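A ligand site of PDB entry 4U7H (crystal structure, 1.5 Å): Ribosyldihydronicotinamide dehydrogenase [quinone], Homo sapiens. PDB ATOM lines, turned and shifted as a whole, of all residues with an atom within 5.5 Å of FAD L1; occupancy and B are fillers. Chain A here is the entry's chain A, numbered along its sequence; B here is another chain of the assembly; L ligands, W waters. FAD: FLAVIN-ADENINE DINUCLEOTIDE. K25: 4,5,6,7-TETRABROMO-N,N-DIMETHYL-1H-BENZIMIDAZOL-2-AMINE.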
ATOM      1  N   HIS A  11     -36.989   4.811  -0.558  1.00  0.00           N
ATOM      2  CA  HIS A  11     -36.002   4.548   0.492  1.00  0.00           C
ATOM      3  C   HIS A  11     -36.302   3.196   1.099  1.00  0.00           C
ATOM      4  O   HIS A  11     -37.466   2.789   1.254  1.00  0.00           O
ATOM      5  CB  HIS A  11     -36.005   5.646   1.560  1.00  0.00           C
ATOM      6  CG  HIS A  11     -34.704   5.741   2.312  1.00  0.00           C
ATOM      7  ND1 HIS A  11     -34.311   4.816   3.261  1.00  0.00           N
ATOM      8  CD2 HIS A  11     -33.734   6.686   2.287  1.00  0.00           C
ATOM      9  CE1 HIS A  11     -33.134   5.173   3.752  1.00  0.00           C
ATOM     10  NE2 HIS A  11     -32.779   6.309   3.198  1.00  0.00           N
ATOM     11  N   LYS A  15     -37.556   4.041   9.025  1.00  0.00           N
ATOM     12  CA  LYS A  15     -37.078   4.965  10.045  1.00  0.00           C
ATOM     13  C   LYS A  15     -36.117   6.024   9.519  1.00  0.00           C
ATOM     14  O   LYS A  15     -35.614   6.847  10.281  1.00  0.00           O
ATOM     15  CB  LYS A  15     -36.384   4.189  11.163  1.00  0.00           C
ATOM     16  CG  LYS A  15     -37.302   3.320  12.017  1.00  0.00           C
ATOM     17  CD  LYS A  15     -36.492   2.501  13.009  1.00  0.00           C
ATOM     18  CE  LYS A  15     -37.300   1.381  13.643  1.00  0.00           C
ATOM     19  NZ  LYS A  15     -36.406   0.406  14.327  1.00  0.00           N
ATOM     20  N   SER A  16     -35.861   6.027   8.223  1.00  0.00           N
ATOM     21  CA  SER A  16     -34.957   7.022   7.649  1.00  0.00           C
ATOM     22  C   SER A  16     -35.479   8.455   7.655  1.00  0.00           C
ATOM     23  O   SER A  16     -36.657   8.671   7.895  1.00  0.00           O
ATOM     24  CB  SER A  16     -34.648   6.632   6.215  1.00  0.00           C
ATOM     25  OG  SER A  16     -35.827   6.700   5.430  1.00  0.00           O
ATOM     26  N   PHE A  17     -34.604   9.416   7.402  1.00  0.00           N
ATOM     27  CA  PHE A  17     -35.018  10.810   7.245  1.00  0.00           C
ATOM     28  C   PHE A  17     -36.014  10.890   6.081  1.00  0.00           C
ATOM     29  O   PHE A  17     -37.032  11.592   6.155  1.00  0.00           O
ATOM     30  CB  PHE A  17     -33.799  11.704   6.993  1.00  0.00           C
ATOM     31  CG  PHE A  17     -34.069  13.160   7.154  1.00  0.00           C
ATOM     32  CD1 PHE A  17     -34.223  13.703   8.411  1.00  0.00           C
ATOM     33  CD2 PHE A  17     -34.136  13.994   6.069  1.00  0.00           C
ATOM     34  CE1 PHE A  17     -34.465  15.044   8.574  1.00  0.00           C
ATOM     35  CE2 PHE A  17     -34.376  15.352   6.223  1.00  0.00           C
ATOM     36  CZ  PHE A  17     -34.530  15.871   7.477  1.00  0.00           C
ATOM     37  N   ASN A  18     -35.751  10.143   5.018  1.00  0.00           N
ATOM     38  CA  ASN A  18     -36.679  10.123   3.870  1.00  0.00           C
ATOM     39  C   ASN A  18     -38.025   9.577   4.311  1.00  0.00           C
ATOM     40  O   ASN A  18     -39.046  10.108   3.924  1.00  0.00           O
ATOM     41  CB  ASN A  18     -36.141   9.278   2.714  1.00  0.00           C
ATOM     42  CG  ASN A  18     -35.334  10.077   1.724  1.00  0.00           C
ATOM     43  OD1 ASN A  18     -35.847  10.562   0.713  1.00  0.00           O
ATOM     44  ND2 ASN A  18     -34.053  10.261   2.034  1.00  0.00           N
ATOM     45  N   GLY A  19     -37.990   8.510   5.094  1.00  0.00           N
ATOM     46  CA  GLY A  19     -39.223   7.923   5.585  1.00  0.00           C
ATOM     47  C   GLY A  19     -40.019   8.935   6.385  1.00  0.00           C
ATOM     48  O   GLY A  19     -41.244   9.027   6.246  1.00  0.00           O
ATOM     49  N   SER A  20     -39.333   9.716   7.211  1.00  0.00           N
ATOM     50  CA  SER A  20     -40.007  10.728   8.009  1.00  0.00           C
ATOM     51  C   SER A  20     -40.582  11.831   7.151  1.00  0.00           C
ATOM     52  O   SER A  20     -41.667  12.331   7.435  1.00  0.00           O
ATOM     53  CB  SER A  20     -39.059  11.313   9.052  1.00  0.00           C
ATOM     54  OG  SER A  20     -38.663  10.333   9.982  1.00  0.00           O
ATOM     55  N   PRO A 102     -33.515   9.962  -1.577  1.00  0.00           N
ATOM     56  CA  PRO A 102     -32.135  10.422  -1.372  1.00  0.00           C
ATOM     57  C   PRO A 102     -31.424  10.548  -2.717  1.00  0.00           C
ATOM     58  O   PRO A 102     -31.624   9.720  -3.609  1.00  0.00           O
ATOM     59  CB  PRO A 102     -31.524   9.292  -0.558  1.00  0.00           C
ATOM     60  CG  PRO A 102     -32.271   8.080  -1.050  1.00  0.00           C
ATOM     61  CD  PRO A 102     -33.647   8.513  -1.343  1.00  0.00           C
ATOM     62  N   LEU A 103     -30.620  11.595  -2.859  1.00  0.00           N
ATOM     63  CA  LEU A 103     -29.846  11.796  -4.071  1.00  0.00           C
ATOM     64  C   LEU A 103     -28.824  10.662  -4.213  1.00  0.00           C
ATOM     65  O   LEU A 103     -28.051  10.424  -3.287  1.00  0.00           O
ATOM     66  CB  LEU A 103     -29.136  13.153  -4.005  1.00  0.00           C
ATOM     67  CG  LEU A 103     -28.561  13.699  -5.308  1.00  0.00           C
ATOM     68  CD1 LEU A 103     -29.644  14.075  -6.265  1.00  0.00           C
ATOM     69  CD2 LEU A 103     -27.664  14.914  -5.043  1.00  0.00           C
ATOM     70  N   TYR A 104     -28.844   9.963  -5.344  1.00  0.00           N
ATOM     71  CA  TYR A 104     -27.863   8.916  -5.654  1.00  0.00           C
ATOM     72  C   TYR A 104     -27.180   9.337  -6.959  1.00  0.00           C
ATOM     73  O   TYR A 104     -27.821   9.378  -8.023  1.00  0.00           O
ATOM     74  CB  TYR A 104     -28.519   7.539  -5.902  1.00  0.00           C
ATOM     75  CG  TYR A 104     -28.844   6.650  -4.712  1.00  0.00           C
ATOM     76  CD1 TYR A 104     -28.941   7.128  -3.417  1.00  0.00           C
ATOM     77  CD2 TYR A 104     -29.039   5.291  -4.927  1.00  0.00           C
ATOM     78  CE1 TYR A 104     -29.270   6.291  -2.369  1.00  0.00           C
ATOM     79  CE2 TYR A 104     -29.355   4.461  -3.905  1.00  0.00           C
ATOM     80  CZ  TYR A 104     -29.448   4.950  -2.632  1.00  0.00           C
ATOM     81  OH  TYR A 104     -29.755   4.076  -1.584  1.00  0.00           O
ATOM     82  N   TRP A 105     -25.901   9.641  -6.876  1.00  0.00           N
ATOM     83  CA  TRP A 105     -25.111   9.991  -8.059  1.00  0.00           C
ATOM     84  C   TRP A 105     -25.747  11.154  -8.855  1.00  0.00           C
ATOM     85  O   TRP A 105     -25.952  11.088 -10.067  1.00  0.00           O
ATOM     86  CB  TRP A 105     -24.835   8.769  -8.923  1.00  0.00           C
ATOM     87  CG  TRP A 105     -23.908   7.766  -8.266  1.00  0.00           C
ATOM     88  CD1 TRP A 105     -24.155   6.454  -8.028  1.00  0.00           C
ATOM     89  CD2 TRP A 105     -22.590   8.025  -7.761  1.00  0.00           C
ATOM     90  NE1 TRP A 105     -23.060   5.863  -7.417  1.00  0.00           N
ATOM     91  CE2 TRP A 105     -22.082   6.809  -7.286  1.00  0.00           C
ATOM     92  CE3 TRP A 105     -21.775   9.165  -7.723  1.00  0.00           C
ATOM     93  CZ2 TRP A 105     -20.800   6.700  -6.712  1.00  0.00           C
ATOM     94  CZ3 TRP A 105     -20.501   9.052  -7.181  1.00  0.00           C
ATOM     95  CH2 TRP A 105     -20.036   7.826  -6.667  1.00  0.00           C
ATOM     96  N   PHE A 106     -26.098  12.194  -8.095  1.00  0.00           N
ATOM     97  CA  PHE A 106     -26.628  13.455  -8.640  1.00  0.00           C
ATOM     98  C   PHE A 106     -27.947  13.201  -9.375  1.00  0.00           C
ATOM     99  O   PHE A 106     -28.323  13.930 -10.305  1.00  0.00           O
ATOM    100  CB  PHE A 106     -25.650  14.125  -9.628  1.00  0.00           C
ATOM    101  CG  PHE A 106     -24.546  14.986  -9.006  1.00  0.00           C
ATOM    102  CD1 PHE A 106     -23.887  14.641  -7.849  1.00  0.00           C
ATOM    103  CD2 PHE A 106     -24.152  16.149  -9.657  1.00  0.00           C
ATOM    104  CE1 PHE A 106     -22.865  15.456  -7.331  1.00  0.00           C
ATOM    105  CE2 PHE A 106     -23.126  16.950  -9.163  1.00  0.00           C
ATOM    106  CZ  PHE A 106     -22.512  16.628  -7.994  1.00  0.00           C
ATOM    107  N   SER A 107     -28.664  12.149  -8.963  1.00  0.00           N
ATOM    108  CA  SER A 107     -29.896  11.731  -9.627  1.00  0.00           C
ATOM    109  C   SER A 107     -30.779  10.945  -8.649  1.00  0.00           C
ATOM    110  O   SER A 107     -30.545  10.947  -7.446  1.00  0.00           O
ATOM    111  CB  SER A 107     -29.529  10.927 -10.868  1.00  0.00           C
ATOM    112  OG  SER A 107     -30.624  10.594 -11.691  1.00  0.00           O
ATOM    113  N   THR A 147     -33.072  14.524  -0.508  1.00  0.00           N
ATOM    114  CA  THR A 147     -32.110  14.640   0.569  1.00  0.00           C
ATOM    115  C   THR A 147     -30.715  14.346   0.003  1.00  0.00           C
ATOM    116  O   THR A 147     -30.572  13.566  -0.950  1.00  0.00           O
ATOM    117  CB  THR A 147     -32.411  13.661   1.699  1.00  0.00           C
ATOM    118  OG1 THR A 147     -32.267  12.302   1.244  1.00  0.00           O
ATOM    119  CG2 THR A 147     -33.841  13.844   2.221  1.00  0.00           C
ATOM    120  N   THR A 148     -29.712  14.934   0.624  1.00  0.00           N
ATOM    121  CA  THR A 148     -28.337  14.807   0.134  1.00  0.00           C
ATOM    122  C   THR A 148     -27.379  14.411   1.226  1.00  0.00           C
ATOM    123  O   THR A 148     -27.621  14.583   2.406  1.00  0.00           O
ATOM    124  CB  THR A 148     -27.803  16.132  -0.416  1.00  0.00           C
ATOM    125  OG1 THR A 148     -27.658  17.063   0.663  1.00  0.00           O
ATOM    126  CG2 THR A 148     -28.732  16.693  -1.469  1.00  0.00           C
ATOM    127  N   GLY A 149     -26.246  13.876   0.799  1.00  0.00           N
ATOM    128  CA  GLY A 149     -25.105  13.667   1.677  1.00  0.00           C
ATOM    129  C   GLY A 149     -24.344  14.979   1.817  1.00  0.00           C
ATOM    130  O   GLY A 149     -23.892  15.327   2.898  1.00  0.00           O
ATOM    131  N   GLY A 150     -24.216  15.723   0.725  1.00  0.00           N
ATOM    132  CA  GLY A 150     -23.461  16.960   0.701  1.00  0.00           C
ATOM    133  C   GLY A 150     -24.193  18.148   1.305  1.00  0.00           C
ATOM    134  O   GLY A 150     -25.429  18.195   1.341  1.00  0.00           O
ATOM    135  N   TYR A 155     -22.995  22.485  -2.750  1.00  0.00           N
ATOM    136  CA  TYR A 155     -23.907  22.606  -3.864  1.00  0.00           C
ATOM    137  C   TYR A 155     -24.140  24.072  -4.263  1.00  0.00           C
ATOM    138  O   TYR A 155     -25.286  24.531  -4.398  1.00  0.00           O
ATOM    139  CB  TYR A 155     -25.226  21.890  -3.571  1.00  0.00           C
ATOM    140  CG  TYR A 155     -25.106  20.385  -3.660  1.00  0.00           C
ATOM    141  CD1 TYR A 155     -25.062  19.768  -4.905  1.00  0.00           C
ATOM    142  CD2 TYR A 155     -25.026  19.598  -2.524  1.00  0.00           C
ATOM    143  CE1 TYR A 155     -24.945  18.400  -5.011  1.00  0.00           C
ATOM    144  CE2 TYR A 155     -24.927  18.229  -2.616  1.00  0.00           C
ATOM    145  CZ  TYR A 155     -24.883  17.636  -3.859  1.00  0.00           C
ATOM    146  OH  TYR A 155     -24.768  16.277  -3.994  1.00  0.00           O
ATOM    147  N   ASN A 161     -19.496  20.570  -5.984  1.00  0.00           N
ATOM    148  CA  ASN A 161     -20.583  19.884  -6.656  1.00  0.00           C
ATOM    149  C   ASN A 161     -21.339  20.719  -7.671  1.00  0.00           C
ATOM    150  O   ASN A 161     -22.172  20.186  -8.396  1.00  0.00           O
ATOM    151  CB  ASN A 161     -21.602  19.345  -5.640  1.00  0.00           C
ATOM    152  CG  ASN A 161     -21.021  18.319  -4.700  1.00  0.00           C
ATOM    153  OD1 ASN A 161     -20.052  17.618  -5.019  1.00  0.00           O
ATOM    154  ND2 ASN A 161     -21.615  18.208  -3.521  1.00  0.00           N
ATOM    155  N   PRO A 192     -28.823  15.648   6.039  1.00  0.00           N
ATOM    156  CA  PRO A 192     -29.405  15.328   7.341  1.00  0.00           C
ATOM    157  C   PRO A 192     -28.483  14.480   8.231  1.00  0.00           C
ATOM    158  O   PRO A 192     -28.531  14.610   9.452  1.00  0.00           O
ATOM    159  CB  PRO A 192     -30.670  14.538   6.977  1.00  0.00           C
ATOM    160  CG  PRO A 192     -30.360  13.958   5.614  1.00  0.00           C
ATOM    161  CD  PRO A 192     -29.573  15.033   4.934  1.00  0.00           C
ATOM    162  N   GLU A 193     -27.644  13.627   7.637  1.00  0.00           N
ATOM    163  CA  GLU A 193     -26.749  12.789   8.434  1.00  0.00           C
ATOM    164  C   GLU A 193     -25.746  13.644   9.220  1.00  0.00           C
ATOM    165  O   GLU A 193     -25.279  13.245  10.282  1.00  0.00           O
ATOM    166  CB  GLU A 193     -26.003  11.765   7.558  1.00  0.00           C
ATOM    167  CG  GLU A 193     -26.894  10.651   6.947  1.00  0.00           C
ATOM    168  CD  GLU A 193     -26.239   9.893   5.782  1.00  0.00           C
ATOM    169  OE1 GLU A 193     -26.201  10.461   4.663  1.00  0.00           O
ATOM    170  OE2 GLU A 193     -25.783   8.744   5.985  1.00  0.00           O
ATOM    171  N   GLU A 197     -29.936  16.966  15.491  1.00  0.00           N
ATOM    172  CA  GLU A 197     -31.368  16.674  15.577  1.00  0.00           C
ATOM    173  C   GLU A 197     -32.188  17.958  15.480  1.00  0.00           C
ATOM    174  O   GLU A 197     -33.230  17.989  14.845  1.00  0.00           O
ATOM    175  CB  GLU A 197     -31.732  15.941  16.864  1.00  0.00           C
ATOM    176  CG  GLU A 197     -31.917  14.447  16.674  1.00  0.00           C
ATOM    177  CD  GLU A 197     -32.928  13.873  17.646  1.00  0.00           C
ATOM    178  OE1 GLU A 197     -32.971  14.329  18.799  1.00  0.00           O
ATOM    179  OE2 GLU A 197     -33.689  12.963  17.233  1.00  0.00           O
ATOM    180  N   ARG A 200     -32.362  18.879  11.973  1.00  0.00           N
ATOM    181  CA  ARG A 200     -33.146  17.864  11.288  1.00  0.00           C
ATOM    182  C   ARG A 200     -34.626  18.107  11.525  1.00  0.00           C
ATOM    183  O   ARG A 200     -35.433  18.038  10.588  1.00  0.00           O
ATOM    184  CB  ARG A 200     -32.776  16.467  11.803  1.00  0.00           C
ATOM    185  CG  ARG A 200     -31.416  15.944  11.353  1.00  0.00           C
ATOM    186  CD  ARG A 200     -31.206  14.533  11.921  1.00  0.00           C
ATOM    187  NE  ARG A 200     -29.801  14.265  12.253  1.00  0.00           N
ATOM    188  CZ  ARG A 200     -29.398  13.654  13.352  1.00  0.00           C
ATOM    189  NH1 ARG A 200     -30.260  13.211  14.255  1.00  0.00           N
ATOM    190  NH2 ARG A 200     -28.099  13.466  13.557  1.00  0.00           N
ATOM    191  N   LYS A 201     -35.002  18.363  12.774  1.00  0.00           N
ATOM    192  CA  LYS A 201     -36.394  18.624  13.083  1.00  0.00           C
ATOM    193  C   LYS A 201     -36.838  19.884  12.334  1.00  0.00           C
ATOM    194  O   LYS A 201     -37.991  19.975  11.883  1.00  0.00           O
ATOM    195  CB  LYS A 201     -36.632  18.741  14.594  1.00  0.00           C
ATOM    196  CG  LYS A 201     -35.829  19.867  15.255  1.00  0.00           C
ATOM    197  CD  LYS A 201     -36.274  20.201  16.686  1.00  0.00           C
ATOM    198  CE  LYS A 201     -35.668  19.260  17.731  1.00  0.00           C
ATOM    199  NZ  LYS A 201     -35.954  19.714  19.118  1.00  0.00           N
ATOM    200  N   VAL A 204     -37.561  18.929   8.662  1.00  0.00           N
ATOM    201  CA  VAL A 204     -38.847  18.233   8.609  1.00  0.00           C
ATOM    202  C   VAL A 204     -39.974  19.255   8.776  1.00  0.00           C
ATOM    203  O   VAL A 204     -40.963  19.221   8.048  1.00  0.00           O
ATOM    204  CB  VAL A 204     -38.921  17.144   9.677  1.00  0.00           C
ATOM    205  CG1 VAL A 204     -40.289  16.488   9.685  1.00  0.00           C
ATOM    206  CG2 VAL A 204     -37.810  16.121   9.482  1.00  0.00           C
ATOM    207  N   ASN B  66     -28.943   1.626   6.589  1.00  0.00           N
ATOM    208  CA  ASN B  66     -28.335   2.753   5.866  1.00  0.00           C
ATOM    209  C   ASN B  66     -27.466   2.169   4.751  1.00  0.00           C
ATOM    210  O   ASN B  66     -26.385   1.620   5.005  1.00  0.00           O
ATOM    211  CB  ASN B  66     -27.489   3.575   6.844  1.00  0.00           C
ATOM    212  CG  ASN B  66     -26.857   4.812   6.229  1.00  0.00           C
ATOM    213  OD1 ASN B  66     -26.266   4.770   5.147  1.00  0.00           O
ATOM    214  ND2 ASN B  66     -27.007   5.940   6.913  1.00  0.00           N
ATOM    215  N   TYR B  67     -27.952   2.216   3.509  1.00  0.00           N
ATOM    216  CA  TYR B  67     -27.279   1.532   2.404  1.00  0.00           C
ATOM    217  C   TYR B  67     -25.818   1.950   2.240  1.00  0.00           C
ATOM    218  O   TYR B  67     -24.942   1.100   2.073  1.00  0.00           O
ATOM    219  CB  TYR B  67     -28.031   1.744   1.083  1.00  0.00           C
ATOM    220  CG  TYR B  67     -27.470   0.912  -0.044  1.00  0.00           C
ATOM    221  CD1 TYR B  67     -27.837  -0.445  -0.177  1.00  0.00           C
ATOM    222  CD2 TYR B  67     -26.568   1.420  -0.967  1.00  0.00           C
ATOM    223  CE1 TYR B  67     -27.338  -1.226  -1.196  1.00  0.00           C
ATOM    224  CE2 TYR B  67     -26.083   0.639  -1.988  1.00  0.00           C
ATOM    225  CZ  TYR B  67     -26.460  -0.675  -2.106  1.00  0.00           C
ATOM    226  OH  TYR B  67     -25.944  -1.446  -3.102  1.00  0.00           O
ATOM    227  N   GLY B  68     -25.551   3.250   2.289  1.00  0.00           N
ATOM    228  CA  GLY B  68     -24.197   3.751   2.198  1.00  0.00           C
ATOM    229  C   GLY B  68     -23.269   3.182   3.256  1.00  0.00           C
ATOM    230  O   GLY B  68     -22.181   2.683   2.956  1.00  0.00           O
ATOM    231  N   ASP B 117     -24.990   2.850  -8.982  1.00  0.00           N
ATOM    232  CA  ASP B 117     -25.352   2.913  -7.578  1.00  0.00           C
ATOM    233  C   ASP B 117     -24.693   1.811  -6.746  1.00  0.00           C
ATOM    234  O   ASP B 117     -24.267   2.044  -5.608  1.00  0.00           O
ATOM    235  CB  ASP B 117     -26.871   2.796  -7.366  1.00  0.00           C
ATOM    236  CG  ASP B 117     -27.663   3.937  -7.975  1.00  0.00           C
ATOM    237  OD1 ASP B 117     -27.094   4.998  -8.328  1.00  0.00           O
ATOM    238  OD2 ASP B 117     -28.903   3.731  -8.079  1.00  0.00           O
ATOM    239  N   GLY B 174     -20.761  14.357 -11.539  1.00  0.00           N
ATOM    240  CA  GLY B 174     -21.326  13.860 -10.293  1.00  0.00           C
ATOM    241  C   GLY B 174     -20.925  12.430  -9.989  1.00  0.00           C
ATOM    242  O   GLY B 174     -20.810  12.074  -8.802  1.00  0.00           O
HETATM  243  PA  FAD L   1     -30.772   8.921   7.227  1.00  0.00           P
HETATM  244  O1A FAD L   1     -31.806   7.824   7.167  1.00  0.00           O
HETATM  245  O2A FAD L   1     -29.416   8.337   7.509  1.00  0.00           O
HETATM  246  O5B FAD L   1     -31.159   9.980   8.345  1.00  0.00           O
HETATM  247  C5B FAD L   1     -30.282  10.964   8.835  1.00  0.00           C
HETATM  248  C4B FAD L   1     -30.560  11.042  10.328  1.00  0.00           C
HETATM  249  O4B FAD L   1     -31.803  11.689  10.537  1.00  0.00           O
HETATM  250  C3B FAD L   1     -30.730   9.644  10.893  1.00  0.00           C
HETATM  251  O3B FAD L   1     -29.950   9.495  12.056  1.00  0.00           O
HETATM  252  C2B FAD L   1     -32.189   9.552  11.249  1.00  0.00           C
HETATM  253  O2B FAD L   1     -32.397   8.735  12.382  1.00  0.00           O
HETATM  254  C1B FAD L   1     -32.519  11.002  11.541  1.00  0.00           C
HETATM  255  N9A FAD L   1     -33.969  11.190  11.415  1.00  0.00           N
HETATM  256  C8A FAD L   1     -34.859  10.407  10.765  1.00  0.00           C
HETATM  257  N7A FAD L   1     -36.139  10.927  10.897  1.00  0.00           N
HETATM  258  C5A FAD L   1     -35.984  12.045  11.642  1.00  0.00           C
HETATM  259  C6A FAD L   1     -36.887  12.978  12.116  1.00  0.00           C
HETATM  260  N6A FAD L   1     -38.184  12.856  11.858  1.00  0.00           N
HETATM  261  N1A FAD L   1     -36.409  14.032  12.863  1.00  0.00           N
HETATM  262  C2A FAD L   1     -35.105  14.100  13.126  1.00  0.00           C
HETATM  263  N3A FAD L   1     -34.159  13.248  12.730  1.00  0.00           N
HETATM  264  C4A FAD L   1     -34.645  12.230  11.986  1.00  0.00           C
HETATM  265  N1  FAD L   1     -25.127  12.437  -1.632  1.00  0.00           N
HETATM  266  C2  FAD L   1     -24.881  13.532  -2.419  1.00  0.00           C
HETATM  267  O2  FAD L   1     -24.869  14.653  -1.913  1.00  0.00           O
HETATM  268  N3  FAD L   1     -24.696  13.395  -3.759  1.00  0.00           N
HETATM  269  C4  FAD L   1     -24.716  12.181  -4.378  1.00  0.00           C
HETATM  270  O4  FAD L   1     -24.613  12.157  -5.582  1.00  0.00           O
HETATM  271  C4X FAD L   1     -24.947  11.063  -3.592  1.00  0.00           C
HETATM  272  N5  FAD L   1     -24.947   9.803  -4.167  1.00  0.00           N
HETATM  273  C5X FAD L   1     -25.178   8.684  -3.381  1.00  0.00           C
HETATM  274  C6  FAD L   1     -25.185   7.437  -3.996  1.00  0.00           C
HETATM  275  C7  FAD L   1     -25.448   6.309  -3.235  1.00  0.00           C
HETATM  276  C7M FAD L   1     -25.464   4.960  -3.919  1.00  0.00           C
HETATM  277  C8  FAD L   1     -25.648   6.436  -1.852  1.00  0.00           C
HETATM  278  C8M FAD L   1     -25.921   5.233  -0.996  1.00  0.00           C
HETATM  279  C9  FAD L   1     -25.649   7.695  -1.236  1.00  0.00           C
HETATM  280  C9A FAD L   1     -25.411   8.816  -2.015  1.00  0.00           C
HETATM  281  N10 FAD L   1     -25.404  10.073  -1.445  1.00  0.00           N
HETATM  282  C10 FAD L   1     -25.153  11.186  -2.217  1.00  0.00           C
HETATM  283  C1' FAD L   1     -25.663  10.229   0.026  1.00  0.00           C
HETATM  284  C2' FAD L   1     -27.228  10.267   0.179  1.00  0.00           C
HETATM  285  O2' FAD L   1     -27.920  11.225  -0.631  1.00  0.00           O
HETATM  286  C3' FAD L   1     -27.581  10.490   1.653  1.00  0.00           C
HETATM  287  O3' FAD L   1     -26.983   9.445   2.387  1.00  0.00           O
HETATM  288  C4' FAD L   1     -29.095  10.515   1.920  1.00  0.00           C
HETATM  289  O4' FAD L   1     -29.660  11.611   1.246  1.00  0.00           O
HETATM  290  C5' FAD L   1     -29.413  10.668   3.398  1.00  0.00           C
HETATM  291  O5' FAD L   1     -30.832  10.546   3.574  1.00  0.00           O
HETATM  292  P   FAD L   1     -31.396   9.360   4.450  1.00  0.00           P
HETATM  293  O1P FAD L   1     -30.817   8.036   4.013  1.00  0.00           O
HETATM  294  O2P FAD L   1     -32.915   9.446   4.464  1.00  0.00           O
HETATM  295  O3P FAD L   1     -30.779   9.797   5.887  1.00  0.00           O
HETATM  296  C2  K25 L   2     -21.398  11.991  -3.931  1.00  0.00           C
HETATM  297  C3  K25 L   2     -21.288  13.164  -3.176  1.00  0.00           C
HETATM  298  C4  K25 L   2     -21.342  13.271  -1.805  1.00  0.00           C
HETATM  299  C5  K25 L   2     -21.610  10.788  -3.218  1.00  0.00           C
HETATM  300  N6  K25 L   2     -21.662  11.806   0.257  1.00  0.00           N
HETATM  301  C7  K25 L   2     -21.670  10.857  -1.811  1.00  0.00           C
HETATM  302  C8  K25 L   2     -21.547  12.080  -1.089  1.00  0.00           C
HETATM  303  C13 K25 L   2     -21.848  10.428   0.313  1.00  0.00           C
HETATM  304  N14 K25 L   2     -21.861   9.825  -0.894  1.00  0.00           N
HETATM  305  N15 K25 L   2     -22.011   9.663   1.401  1.00  0.00           N
HETATM  306  C16 K25 L   2     -22.185   8.257   1.231  1.00  0.00           C
HETATM  307  C17 K25 L   2     -22.041  10.205   2.722  1.00  0.00           C
HETATM  308 BR1  K25 L   2     -21.302  12.243  -5.845  1.00  0.00          BR
HETATM  309 BR9  K25 L   2     -21.022  14.822  -3.986  1.00  0.00          BR
HETATM  310 BR10 K25 L   2     -21.100  15.048  -1.017  1.00  0.00          BR
HETATM  311 BR11 K25 L   2     -21.758   9.092  -4.049  1.00  0.00          BR
HETATM  312  O   HOH W   1     -29.297   6.093   4.997  1.00  0.00           O
HETATM  313  O   HOH W   2     -25.013   7.366   1.996  1.00  0.00           O
HETATM  314  O   HOH W   3     -29.724   6.909   1.654  1.00  0.00           O
HETATM  315  O   HOH W   4     -29.058   5.484   9.421  1.00  0.00           O
HETATM  316  O   HOH W   5     -28.000   7.725   9.360  1.00  0.00           O
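Water W5 lies within hydrogen-bond range of an oxygen (O2A) of FAD L1 (2.4 Å) and the side-chain amide nitrogen (ND2) of Asn 66 of chain B (3.2 Å).
Water W1 lies within hydrogen-bond range of an oxygen (O1P) of FAD L1 (2.7 Å) and the side-chain amide nitrogen of Asn 66 of chain B (3.0 Å).
Water W3 lies within hydrogen-bond range of an oxygen (O1P) of FAD L1 (2.8 Å) and a ring nitrogen (NE2) of His 11 (3.5 Å).
Water W4 lies within hydrogen-bond range of ND2 of Asn 66 of chain B (3.3 Å) and O2A of FAD L1 (3.5 Å).
Merely in contact with FAD L1: Arg 200 (3.2 Å), Ser 16 (3.2 Å), Tyr 104 (3.4 Å), Pro 102 (3.5 Å), Asp 117 of chain B (3.6 Å), Lys 15 (3.7 Å), Gly 68 of chain B (3.9 Å), Tyr 67 of chain B (3.9 Å) and Pro 192 (3.995 Å).
23 residues have an atom within 4 Å of FAD L1: His 11, Lys 15, Ser 16, Phe 17, Asn 18, Ser 20, Pro 102, Leu 103, Tyr 104, Trp 105, Phe 106, Thr 147, Thr 148, Gly 149, Gly 150, Tyr 155, Pro 192, Glu 193, Arg 200, Asn 66 of chain B, Tyr 67 of chain B, Gly 68 of chain B and Asp 117 of chain B.
A ring nitrogen (ND1) of His 11 lies within hydrogen-bond range of the side-chain hydroxyl of Ser 16.
The backbone NH of Gly 19 is in hydrogen-bond range of the side-chain hydroxyl of Ser 16, at 2.8 Å.
The backbone NH (N) of Asn 18 lies close to the side-chain hydroxyl (OG) of Ser 16.
O of Ser 16 is in hydrogen-bond range of OG of Ser 20.
The backbone carbonyl oxygen (O) of Thr 147 lies within hydrogen-bond range of the backbone NH (N) of Leu 103, 2.7 Å away.
The side-chain amide nitrogen (ND2) of Asn 18 is in hydrogen-bond range of the side-chain hydroxyl (OG1) of Thr 147, 2.8 Å away.
The side-chain amide nitrogen of Asn 66 of chain B lies within hydrogen-bond range of the side-chain carboxylate of Glu 193, 3.2 Å away.
The guanidinium group (NE) of Arg 200 lies within hydrogen-bond range of the backbone carbonyl oxygen (O) of Pro 192, at 3.1 Å.
The backbone carbonyl oxygen (O) of Leu 103 lies within hydrogen-bond range of an oxygen (O2') of FAD L1, 2.8 Å away.
An oxygen (O3') of FAD L1 sits at hydrogen-bond distance from the side-chain carboxylate (OE1) of Glu 193, at 2.6 Å.
An oxygen (O4) of FAD L1 sits at hydrogen-bond distance from the backbone NH of Phe 106.
The backbone NH (N) of Gly 149 sits at hydrogen-bond distance from a nitrogen (N1) of FAD L1 (3.0 Å).
N5 of FAD L1 is in hydrogen-bond range of N of Trp 105, at 2.9 Å.
The side-chain amide nitrogen of Asn 18 lies within hydrogen-bond range of an oxygen (O2P) of FAD L1.
O4' of FAD L1 sits at hydrogen-bond distance from OG1 of Thr 147, at 2.7 Å.
The backbone NH of Gly 150 sits at hydrogen-bond distance from an oxygen (O2) of FAD L1 (2.9 Å).
The backbone NH (N) of Phe 17 sits at hydrogen-bond distance from an oxygen (O1A) of FAD L1 (3.2 Å).
NE2 of His 11 sits at hydrogen-bond distance from O1P of FAD L1, 2.7 Å away.
O2A of FAD L1 sits at hydrogen-bond distance from ND2 of Asn 66 of chain B.
The side-chain hydroxyl (OH) of Tyr 155 lies within hydrogen-bond range of an oxygen (O2) of FAD L1.
N of Asn 18 is in hydrogen-bond range of O2P of FAD L1.
OG of Ser 20 is in hydrogen-bond range of N7A of FAD L1 (2.7 Å).
O4' of FAD L1 sits at hydrogen-bond distance from N of Thr 148, 3.4 Å away.
The backbone carbonyl oxygen (O) of Thr 147 is in hydrogen-bond range of an oxygen (O4') of FAD L1 (3.1 Å).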
